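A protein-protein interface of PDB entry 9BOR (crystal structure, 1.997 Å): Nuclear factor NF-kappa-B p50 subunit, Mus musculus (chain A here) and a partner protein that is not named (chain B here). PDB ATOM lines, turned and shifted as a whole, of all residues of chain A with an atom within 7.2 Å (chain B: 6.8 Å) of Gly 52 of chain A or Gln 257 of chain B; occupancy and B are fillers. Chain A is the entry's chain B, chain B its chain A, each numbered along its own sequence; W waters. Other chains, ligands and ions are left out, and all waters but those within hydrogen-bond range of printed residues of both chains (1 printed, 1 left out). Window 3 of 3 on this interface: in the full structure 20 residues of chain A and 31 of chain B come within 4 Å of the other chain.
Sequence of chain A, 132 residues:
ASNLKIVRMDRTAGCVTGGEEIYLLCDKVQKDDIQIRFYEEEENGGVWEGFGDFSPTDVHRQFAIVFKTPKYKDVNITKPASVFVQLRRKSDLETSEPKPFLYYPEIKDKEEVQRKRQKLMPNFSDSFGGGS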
ATOM      1  N   ILE A  34     -27.569 -31.464 -10.234  1.00  0.00           N
ATOM      2  CA  ILE A  34     -27.196 -32.683  -9.529  1.00  0.00           C
ATOM      3  C   ILE A  34     -26.832 -32.400  -8.074  1.00  0.00           C
ATOM      4  O   ILE A  34     -26.226 -31.378  -7.749  1.00  0.00           O
ATOM      5  CB  ILE A  34     -26.027 -33.423 -10.254  1.00  0.00           C
ATOM      6  CG1 ILE A  34     -25.908 -34.867  -9.747  1.00  0.00           C
ATOM      7  CG2 ILE A  34     -24.715 -32.647 -10.146  1.00  0.00           C
ATOM      8  CD1 ILE A  34     -27.149 -35.702 -10.043  1.00  0.00           C
ATOM      9  N   GLN A  35     -27.265 -33.303  -7.201  1.00  0.00           N
ATOM     10  CA  GLN A  35     -26.945 -33.263  -5.781  1.00  0.00           C
ATOM     11  C   GLN A  35     -26.352 -34.595  -5.360  1.00  0.00           C
ATOM     12  O   GLN A  35     -26.633 -35.625  -5.975  1.00  0.00           O
ATOM     13  CB  GLN A  35     -28.188 -33.003  -4.930  1.00  0.00           C
ATOM     14  CG  GLN A  35     -28.725 -31.597  -4.947  1.00  0.00           C
ATOM     15  CD  GLN A  35     -29.920 -31.453  -4.023  1.00  0.00           C
ATOM     16  OE1 GLN A  35     -30.700 -32.394  -3.844  1.00  0.00           O
ATOM     17  NE2 GLN A  35     -30.052 -30.287  -3.406  1.00  0.00           N
ATOM     18  N   ILE A  36     -25.559 -34.569  -4.296  1.00  0.00           N
ATOM     19  CA  ILE A  36     -25.099 -35.793  -3.661  1.00  0.00           C
ATOM     20  C   ILE A  36     -25.634 -35.790  -2.241  1.00  0.00           C
ATOM     21  O   ILE A  36     -25.287 -34.923  -1.443  1.00  0.00           O
ATOM     22  CB  ILE A  36     -23.575 -35.907  -3.658  1.00  0.00           C
ATOM     23  CG1 ILE A  36     -23.060 -35.896  -5.097  1.00  0.00           C
ATOM     24  CG2 ILE A  36     -23.125 -37.192  -2.917  1.00  0.00           C
ATOM     25  CD1 ILE A  36     -21.572 -35.784  -5.198  1.00  0.00           C
ATOM     26  N   ARG A  37     -26.506 -36.745  -1.949  1.00  0.00           N
ATOM     27  CA  ARG A  37     -27.236 -36.758  -0.689  1.00  0.00           C
ATOM     28  C   ARG A  37     -26.806 -37.927   0.177  1.00  0.00           C
ATOM     29  O   ARG A  37     -26.896 -39.078  -0.242  1.00  0.00           O
ATOM     30  CB  ARG A  37     -28.739 -36.824  -0.955  1.00  0.00           C
ATOM     31  CG  ARG A  37     -29.618 -36.924   0.275  1.00  0.00           C
ATOM     32  CD  ARG A  37     -31.097 -36.879  -0.154  1.00  0.00           C
ATOM     33  NE  ARG A  37     -32.006 -37.023   0.979  1.00  0.00           N
ATOM     34  CZ  ARG A  37     -32.720 -38.112   1.249  1.00  0.00           C
ATOM     35  NH1 ARG A  37     -32.653 -39.177   0.456  1.00  0.00           N
ATOM     36  NH2 ARG A  37     -33.507 -38.133   2.319  1.00  0.00           N
ATOM     37  N   PHE A  38     -26.313 -37.610   1.370  1.00  0.00           N
ATOM     38  CA  PHE A  38     -26.033 -38.594   2.410  1.00  0.00           C
ATOM     39  C   PHE A  38     -27.274 -38.656   3.278  1.00  0.00           C
ATOM     40  O   PHE A  38     -27.828 -37.612   3.619  1.00  0.00           O
ATOM     41  CB  PHE A  38     -24.803 -38.200   3.248  1.00  0.00           C
ATOM     42  CG  PHE A  38     -23.494 -38.263   2.490  1.00  0.00           C
ATOM     43  CD1 PHE A  38     -22.501 -39.154   2.869  1.00  0.00           C
ATOM     44  CD2 PHE A  38     -23.258 -37.426   1.408  1.00  0.00           C
ATOM     45  CE1 PHE A  38     -21.297 -39.212   2.181  1.00  0.00           C
ATOM     46  CE2 PHE A  38     -22.061 -37.483   0.710  1.00  0.00           C
ATOM     47  CZ  PHE A  38     -21.077 -38.381   1.100  1.00  0.00           C
ATOM     48  N   GLY A  50     -27.600 -34.992   4.609  1.00  0.00           N
ATOM     49  CA  GLY A  50     -26.505 -34.050   4.473  1.00  0.00           C
ATOM     50  C   GLY A  50     -26.104 -34.048   3.012  1.00  0.00           C
ATOM     51  O   GLY A  50     -26.254 -35.067   2.332  1.00  0.00           O
ATOM     52  N   PHE A  51     -25.617 -32.922   2.509  1.00  0.00           N
ATOM     53  CA  PHE A  51     -25.297 -32.856   1.089  1.00  0.00           C
ATOM     54  C   PHE A  51     -23.816 -32.646   0.835  1.00  0.00           C
ATOM     55  O   PHE A  51     -23.151 -31.889   1.541  1.00  0.00           O
ATOM     56  CB  PHE A  51     -26.132 -31.756   0.414  1.00  0.00           C
ATOM     57  CG  PHE A  51     -27.596 -32.064   0.405  1.00  0.00           C
ATOM     58  CD1 PHE A  51     -28.163 -32.767  -0.645  1.00  0.00           C
ATOM     59  CD2 PHE A  51     -28.395 -31.716   1.484  1.00  0.00           C
ATOM     60  CE1 PHE A  51     -29.510 -33.084  -0.639  1.00  0.00           C
ATOM     61  CE2 PHE A  51     -29.742 -32.030   1.496  1.00  0.00           C
ATOM     62  CZ  PHE A  51     -30.301 -32.713   0.436  1.00  0.00           C
ATOM     63  N   GLY A  52     -23.300 -33.346  -0.171  1.00  0.00           N
ATOM     64  CA  GLY A  52     -21.937 -33.141  -0.611  1.00  0.00           C
ATOM     65  C   GLY A  52     -21.758 -31.707  -1.069  1.00  0.00           C
ATOM     66  O   GLY A  52     -22.645 -31.131  -1.709  1.00  0.00           O
ATOM     67  N   ASP A  53     -20.612 -31.131  -0.731  1.00  0.00           N
ATOM     68  CA  ASP A  53     -20.328 -29.730  -1.025  1.00  0.00           C
ATOM     69  C   ASP A  53     -19.460 -29.628  -2.273  1.00  0.00           C
ATOM     70  O   ASP A  53     -18.322 -30.099  -2.277  1.00  0.00           O
ATOM     71  CB  ASP A  53     -19.642 -29.077   0.187  1.00  0.00           C
ATOM     72  CG  ASP A  53     -19.197 -27.644  -0.076  1.00  0.00           C
ATOM     73  OD1 ASP A  53     -19.939 -26.891  -0.733  1.00  0.00           O
ATOM     74  OD2 ASP A  53     -18.099 -27.269   0.388  1.00  0.00           O
ATOM     75  N   PHE A  54     -20.006 -29.041  -3.338  1.00  0.00           N
ATOM     76  CA  PHE A  54     -19.257 -28.836  -4.580  1.00  0.00           C
ATOM     77  C   PHE A  54     -19.894 -27.747  -5.429  1.00  0.00           C
ATOM     78  O   PHE A  54     -21.085 -27.483  -5.325  1.00  0.00           O
ATOM     79  CB  PHE A  54     -19.160 -30.134  -5.403  1.00  0.00           C
ATOM     80  CG  PHE A  54     -20.487 -30.656  -5.888  1.00  0.00           C
ATOM     81  CD1 PHE A  54     -20.930 -30.380  -7.183  1.00  0.00           C
ATOM     82  CD2 PHE A  54     -21.291 -31.423  -5.055  1.00  0.00           C
ATOM     83  CE1 PHE A  54     -22.154 -30.859  -7.633  1.00  0.00           C
ATOM     84  CE2 PHE A  54     -22.513 -31.911  -5.495  1.00  0.00           C
ATOM     85  CZ  PHE A  54     -22.948 -31.629  -6.787  1.00  0.00           C
ATOM     86  N   SER A  55     -19.088 -27.114  -6.269  1.00  0.00           N
ATOM     87  CA  SER A  55     -19.615 -26.175  -7.246  1.00  0.00           C
ATOM     88  C   SER A  55     -19.699 -26.886  -8.587  1.00  0.00           C
ATOM     89  O   SER A  55     -19.014 -27.887  -8.797  1.00  0.00           O
ATOM     90  CB  SER A  55     -18.742 -24.918  -7.324  1.00  0.00           C
ATOM     91  OG  SER A  55     -17.574 -25.134  -8.094  1.00  0.00           O
ATOM     92  N   PRO A  56     -20.561 -26.391  -9.488  1.00  0.00           N
ATOM     93  CA  PRO A  56     -20.710 -26.964 -10.832  1.00  0.00           C
ATOM     94  C   PRO A  56     -19.388 -27.217 -11.561  1.00  0.00           C
ATOM     95  O   PRO A  56     -19.307 -28.175 -12.332  1.00  0.00           O
ATOM     96  CB  PRO A  56     -21.541 -25.900 -11.557  1.00  0.00           C
ATOM     97  CG  PRO A  56     -22.417 -25.349 -10.475  1.00  0.00           C
ATOM     98  CD  PRO A  56     -21.578 -25.354  -9.220  1.00  0.00           C
ATOM     99  N   PHE A  67     -16.202 -33.660  -4.587  1.00  0.00           N
ATOM    100  CA  PHE A  67     -17.007 -32.960  -3.590  1.00  0.00           C
ATOM    101  C   PHE A  67     -16.475 -33.187  -2.189  1.00  0.00           C
ATOM    102  O   PHE A  67     -15.686 -34.099  -1.962  1.00  0.00           O
ATOM    103  CB  PHE A  67     -18.467 -33.419  -3.664  1.00  0.00           C
ATOM    104  CG  PHE A  67     -18.677 -34.845  -3.214  1.00  0.00           C
ATOM    105  CD1 PHE A  67     -18.419 -35.901  -4.076  1.00  0.00           C
ATOM    106  CD2 PHE A  67     -19.115 -35.127  -1.922  1.00  0.00           C
ATOM    107  CE1 PHE A  67     -18.608 -37.218  -3.666  1.00  0.00           C
ATOM    108  CE2 PHE A  67     -19.301 -36.429  -1.506  1.00  0.00           C
ATOM    109  CZ  PHE A  67     -19.046 -37.481  -2.380  1.00  0.00           C
ATOM    110  N   LYS A  68     -16.911 -32.352  -1.254  1.00  0.00           N
ATOM    111  CA  LYS A  68     -16.563 -32.545   0.150  1.00  0.00           C
ATOM    112  C   LYS A  68     -17.744 -33.119   0.917  1.00  0.00           C
ATOM    113  O   LYS A  68     -18.889 -32.691   0.745  1.00  0.00           O
ATOM    114  CB  LYS A  68     -16.097 -31.231   0.784  1.00  0.00           C
ATOM    115  CG  LYS A  68     -14.786 -30.718   0.196  1.00  0.00           C
ATOM    116  CD  LYS A  68     -14.288 -29.477   0.916  1.00  0.00           C
ATOM    117  CE  LYS A  68     -13.079 -28.882   0.207  1.00  0.00           C
ATOM    118  NZ  LYS A  68     -13.409 -28.440  -1.184  1.00  0.00           N
ATOM    119  N   THR A  69     -17.451 -34.098   1.768  1.00  0.00           N
ATOM    120  CA  THR A  69     -18.465 -34.737   2.589  1.00  0.00           C
ATOM    121  C   THR A  69     -19.154 -33.749   3.508  1.00  0.00           C
ATOM    122  O   THR A  69     -18.530 -32.803   3.987  1.00  0.00           O
ATOM    123  CB  THR A  69     -17.858 -35.840   3.469  1.00  0.00           C
ATOM    124  OG1 THR A  69     -16.755 -35.295   4.200  1.00  0.00           O
ATOM    125  CG2 THR A  69     -17.381 -37.005   2.615  1.00  0.00           C
ATOM    126  N   PRO A  70     -20.444 -33.978   3.771  1.00  0.00           N
ATOM    127  CA  PRO A  70     -21.113 -33.197   4.810  1.00  0.00           C
ATOM    128  C   PRO A  70     -20.681 -33.659   6.191  1.00  0.00           C
ATOM    129  O   PRO A  70     -20.199 -34.782   6.361  1.00  0.00           O
ATOM    130  CB  PRO A  70     -22.592 -33.494   4.581  1.00  0.00           C
ATOM    131  CG  PRO A  70     -22.598 -34.871   3.985  1.00  0.00           C
ATOM    132  CD  PRO A  70     -21.351 -34.948   3.133  1.00  0.00           C
ATOM    133  N   VAL A  85     -25.517 -43.081   0.567  1.00  0.00           N
ATOM    134  CA  VAL A  85     -25.252 -41.917  -0.256  1.00  0.00           C
ATOM    135  C   VAL A  85     -25.867 -42.166  -1.632  1.00  0.00           C
ATOM    136  O   VAL A  85     -25.794 -43.273  -2.166  1.00  0.00           O
ATOM    137  CB  VAL A  85     -23.733 -41.607  -0.355  1.00  0.00           C
ATOM    138  CG1 VAL A  85     -22.970 -42.796  -0.879  1.00  0.00           C
ATOM    139  CG2 VAL A  85     -23.491 -40.386  -1.261  1.00  0.00           C
ATOM    140  N   LYS A  90     -31.878 -32.326  -8.968  1.00  0.00           N
ATOM    141  CA  LYS A  90     -32.634 -31.259  -8.316  1.00  0.00           C
ATOM    142  C   LYS A  90     -33.995 -31.043  -8.967  1.00  0.00           C
ATOM    143  O   LYS A  90     -34.976 -30.779  -8.282  1.00  0.00           O
ATOM    144  CB  LYS A  90     -31.861 -29.941  -8.339  1.00  0.00           C
ATOM    145  CG  LYS A  90     -30.539 -29.942  -7.604  1.00  0.00           C
ATOM    146  CD  LYS A  90     -29.904 -28.577  -7.772  1.00  0.00           C
ATOM    147  CE  LYS A  90     -28.462 -28.549  -7.341  1.00  0.00           C
ATOM    148  NZ  LYS A  90     -27.856 -27.235  -7.697  1.00  0.00           N
ATOM    149  N   GLU B 219     -13.539 -21.086  -2.782  1.00  0.00           N
ATOM    150  CA  GLU B 219     -14.447 -22.226  -2.683  1.00  0.00           C
ATOM    151  C   GLU B 219     -15.438 -22.074  -1.534  1.00  0.00           C
ATOM    152  O   GLU B 219     -16.530 -22.638  -1.568  1.00  0.00           O
ATOM    153  CB  GLU B 219     -13.661 -23.532  -2.496  1.00  0.00           C
ATOM    154  CG  GLU B 219     -12.941 -24.018  -3.729  1.00  0.00           C
ATOM    155  CD  GLU B 219     -12.308 -25.382  -3.521  1.00  0.00           C
ATOM    156  OE1 GLU B 219     -11.791 -25.954  -4.503  1.00  0.00           O
ATOM    157  OE2 GLU B 219     -12.336 -25.883  -2.374  1.00  0.00           O
ATOM    158  N   VAL B 252     -14.926 -19.846  -9.725  1.00  0.00           N
ATOM    159  CA  VAL B 252     -15.374 -20.600  -8.556  1.00  0.00           C
ATOM    160  C   VAL B 252     -16.388 -19.795  -7.747  1.00  0.00           C
ATOM    161  O   VAL B 252     -17.490 -20.272  -7.476  1.00  0.00           O
ATOM    162  CB  VAL B 252     -14.185 -20.993  -7.669  1.00  0.00           C
ATOM    163  CG1 VAL B 252     -14.666 -21.654  -6.374  1.00  0.00           C
ATOM    164  CG2 VAL B 252     -13.243 -21.918  -8.436  1.00  0.00           C
ATOM    165  N   ALA B 253     -16.016 -18.566  -7.391  1.00  0.00           N
ATOM    166  CA  ALA B 253     -16.888 -17.682  -6.616  1.00  0.00           C
ATOM    167  C   ALA B 253     -18.246 -17.460  -7.284  1.00  0.00           C
ATOM    168  O   ALA B 253     -19.283 -17.466  -6.620  1.00  0.00           O
ATOM    169  CB  ALA B 253     -16.201 -16.338  -6.374  1.00  0.00           C
ATOM    170  N   SER B 255     -19.841 -19.394  -9.234  1.00  0.00           N
ATOM    171  CA  SER B 255     -20.581 -20.637  -9.447  1.00  0.00           C
ATOM    172  C   SER B 255     -21.080 -21.334  -8.166  1.00  0.00           C
ATOM    173  O   SER B 255     -21.821 -22.310  -8.249  1.00  0.00           O
ATOM    174  CB  SER B 255     -19.706 -21.624 -10.231  1.00  0.00           C
ATOM    175  OG  SER B 255     -18.602 -22.055  -9.451  1.00  0.00           O
ATOM    176  N   LEU B 256     -20.683 -20.833  -7.000  1.00  0.00           N
ATOM    177  CA  LEU B 256     -20.900 -21.520  -5.718  1.00  0.00           C
ATOM    178  C   LEU B 256     -22.347 -21.883  -5.357  1.00  0.00           C
ATOM    179  O   LEU B 256     -23.288 -21.213  -5.769  1.00  0.00           O
ATOM    180  CB  LEU B 256     -20.346 -20.661  -4.583  1.00  0.00           C
ATOM    181  CG  LEU B 256     -18.833 -20.486  -4.517  1.00  0.00           C
ATOM    182  CD1 LEU B 256     -18.460 -19.576  -3.356  1.00  0.00           C
ATOM    183  CD2 LEU B 256     -18.145 -21.837  -4.387  1.00  0.00           C
ATOM    184  N   GLN B 257     -22.503 -22.953  -4.576  1.00  0.00           N
ATOM    185  CA  GLN B 257     -23.734 -23.185  -3.826  1.00  0.00           C
ATOM    186  C   GLN B 257     -23.941 -21.965  -2.937  1.00  0.00           C
ATOM    187  O   GLN B 257     -22.973 -21.440  -2.376  1.00  0.00           O
ATOM    188  CB  GLN B 257     -23.651 -24.465  -2.983  1.00  0.00           C
ATOM    189  CG  GLN B 257     -23.561 -25.772  -3.765  1.00  0.00           C
ATOM    190  CD  GLN B 257     -23.106 -26.944  -2.903  1.00  0.00           C
ATOM    191  OE1 GLN B 257     -22.387 -26.759  -1.919  1.00  0.00           O
ATOM    192  NE2 GLN B 257     -23.540 -28.155  -3.258  1.00  0.00           N
ATOM    193  N   TYR B 258     -25.180 -21.492  -2.831  1.00  0.00           N
ATOM    194  CA  TYR B 258     -25.442 -20.215  -2.167  1.00  0.00           C
ATOM    195  C   TYR B 258     -24.829 -20.125  -0.774  1.00  0.00           C
ATOM    196  O   TYR B 258     -25.088 -20.951   0.102  1.00  0.00           O
ATOM    197  CB  TYR B 258     -26.945 -19.932  -2.067  1.00  0.00           C
ATOM    198  CG  TYR B 258     -27.233 -18.588  -1.424  1.00  0.00           C
ATOM    199  CD1 TYR B 258     -27.215 -17.418  -2.178  1.00  0.00           C
ATOM    200  CD2 TYR B 258     -27.493 -18.485  -0.058  1.00  0.00           C
ATOM    201  CE1 TYR B 258     -27.460 -16.189  -1.596  1.00  0.00           C
ATOM    202  CE2 TYR B 258     -27.738 -17.259   0.532  1.00  0.00           C
ATOM    203  CZ  TYR B 258     -27.722 -16.115  -0.241  1.00  0.00           C
ATOM    204  OH  TYR B 258     -27.968 -14.895   0.339  1.00  0.00           O
ATOM    205  N   ARG B 259     -23.992 -19.111  -0.605  1.00  0.00           N
ATOM    206  CA  ARG B 259     -23.454 -18.739   0.689  1.00  0.00           C
ATOM    207  C   ARG B 259     -23.803 -17.281   0.918  1.00  0.00           C
ATOM    208  O   ARG B 259     -23.979 -16.523  -0.036  1.00  0.00           O
ATOM    209  CB  ARG B 259     -21.945 -18.958   0.740  1.00  0.00           C
ATOM    210  CG  ARG B 259     -21.543 -20.420   0.834  1.00  0.00           C
ATOM    211  CD  ARG B 259     -20.064 -20.597   0.566  1.00  0.00           C
ATOM    212  NE  ARG B 259     -19.581 -21.922   0.945  1.00  0.00           N
ATOM    213  CZ  ARG B 259     -19.764 -23.022   0.220  1.00  0.00           C
ATOM    214  NH1 ARG B 259     -19.280 -24.184   0.644  1.00  0.00           N
ATOM    215  NH2 ARG B 259     -20.437 -22.963  -0.923  1.00  0.00           N
ATOM    216  N   LEU B 260     -23.913 -16.887   2.178  1.00  0.00           N
ATOM    217  CA  LEU B 260     -24.292 -15.522   2.508  1.00  0.00           C
ATOM    218  C   LEU B 260     -23.203 -14.527   2.092  1.00  0.00           C
ATOM    219  O   LEU B 260     -23.456 -13.333   1.961  1.00  0.00           O
ATOM    220  CB  LEU B 260     -24.605 -15.424   4.003  1.00  0.00           C
ATOM    221  CG  LEU B 260     -25.916 -16.147   4.344  1.00  0.00           C
ATOM    222  CD1 LEU B 260     -26.054 -16.482   5.826  1.00  0.00           C
ATOM    223  CD2 LEU B 260     -27.108 -15.314   3.871  1.00  0.00           C
ATOM    224  N   GLN B 262     -21.270 -15.030  -0.763  1.00  0.00           N
ATOM    225  CA  GLN B 262     -20.952 -15.245  -2.179  1.00  0.00           C
ATOM    226  C   GLN B 262     -20.875 -13.948  -2.980  1.00  0.00           C
ATOM    227  O   GLN B 262     -19.881 -13.689  -3.663  1.00  0.00           O
ATOM    228  CB  GLN B 262     -21.978 -16.170  -2.840  1.00  0.00           C
ATOM    229  CG  GLN B 262     -21.649 -16.473  -4.297  1.00  0.00           C
ATOM    230  CD  GLN B 262     -22.665 -17.386  -4.955  1.00  0.00           C
ATOM    231  OE1 GLN B 262     -23.755 -17.605  -4.424  1.00  0.00           O
ATOM    232  NE2 GLN B 262     -22.312 -17.922  -6.123  1.00  0.00           N
ATOM    233  N   PRO B 291     -25.558 -19.552 -10.942  1.00  0.00           N
ATOM    234  CA  PRO B 291     -26.749 -20.379 -10.716  1.00  0.00           C
ATOM    235  C   PRO B 291     -27.986 -19.765 -11.360  1.00  0.00           C
ATOM    236  O   PRO B 291     -28.008 -18.559 -11.613  1.00  0.00           O
ATOM    237  CB  PRO B 291     -26.870 -20.415  -9.186  1.00  0.00           C
ATOM    238  CG  PRO B 291     -26.105 -19.229  -8.709  1.00  0.00           C
ATOM    239  CD  PRO B 291     -24.983 -19.051  -9.683  1.00  0.00           C
HETATM  240  O   HOH W   1     -25.459 -29.735  -5.496  1.00  0.00           O
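Hydrophobic or aromatic side chains of chain A within 4 Å of the printed part of chain B: Pro 56.
Along chain A the printed residues that touch a printed residue of chain B span positions 52 to 68.
Among the printed residues, 7 pairs touch across the chains.
Of the printed residues of chain A, Glu 219 of chain B touches Lys 68.
Of the printed residues of chain B, Ser 55 of chain A touches Ser 255.
The backbone carbonyl oxygen of Val 252 of chain B is in hydrogen-bond range of the side-chain hydroxyl of Ser 255 of chain B (2.9 Å).
The guanidinium group of Arg 259 of chain B lies within hydrogen-bond range of the backbone carbonyl oxygen of Gln 257 of chain B.
O of Ile 36 of chain A lies within hydrogen-bond range of N of Gly 52 of chain A (2.8 Å).
The backbone carbonyl oxygen (O) of Lys 68 of chain A sits at hydrogen-bond distance from the backbone NH (N) of Asp 53 of chain A (2.8 Å).
Water W1 bridges the backbone carbonyl oxygen (O) of Ile 34 of chain A (2.9 Å) and the side-chain amide nitrogen (NE2) of Gln 257 of chain B (3.3 Å).
Ser 55 of chain A touches Ser 255 of chain B.
Pro 56 of chain A touches Ser 255 of chain B (CD to O, 3.2 Å).
The side-chain amino group (NZ) of Lys 68 of chain A is in salt-bridge range of the side-chain carboxylate (OE2) of Glu 219 of chain B (3.0 Å).
The side-chain amide nitrogen of Gln 257 of chain B sits at hydrogen-bond distance from the backbone carbonyl oxygen of Gly 52 of chain A (3.5 Å).
The side-chain carboxylate (OD1) of Asp 53 of chain A sits close to the side-chain amide oxygen (OE1) of Gln 257 of chain B.
The backbone carbonyl oxygen (O) of Phe 54 of chain A sits close to the side-chain amide nitrogen (NE2) of Gln 257 of chain B.
The guanidinium group (NH1) of Arg 259 of chain B lies within salt-bridge range of the side-chain carboxylate (OD1) of Asp 53 of chain A.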
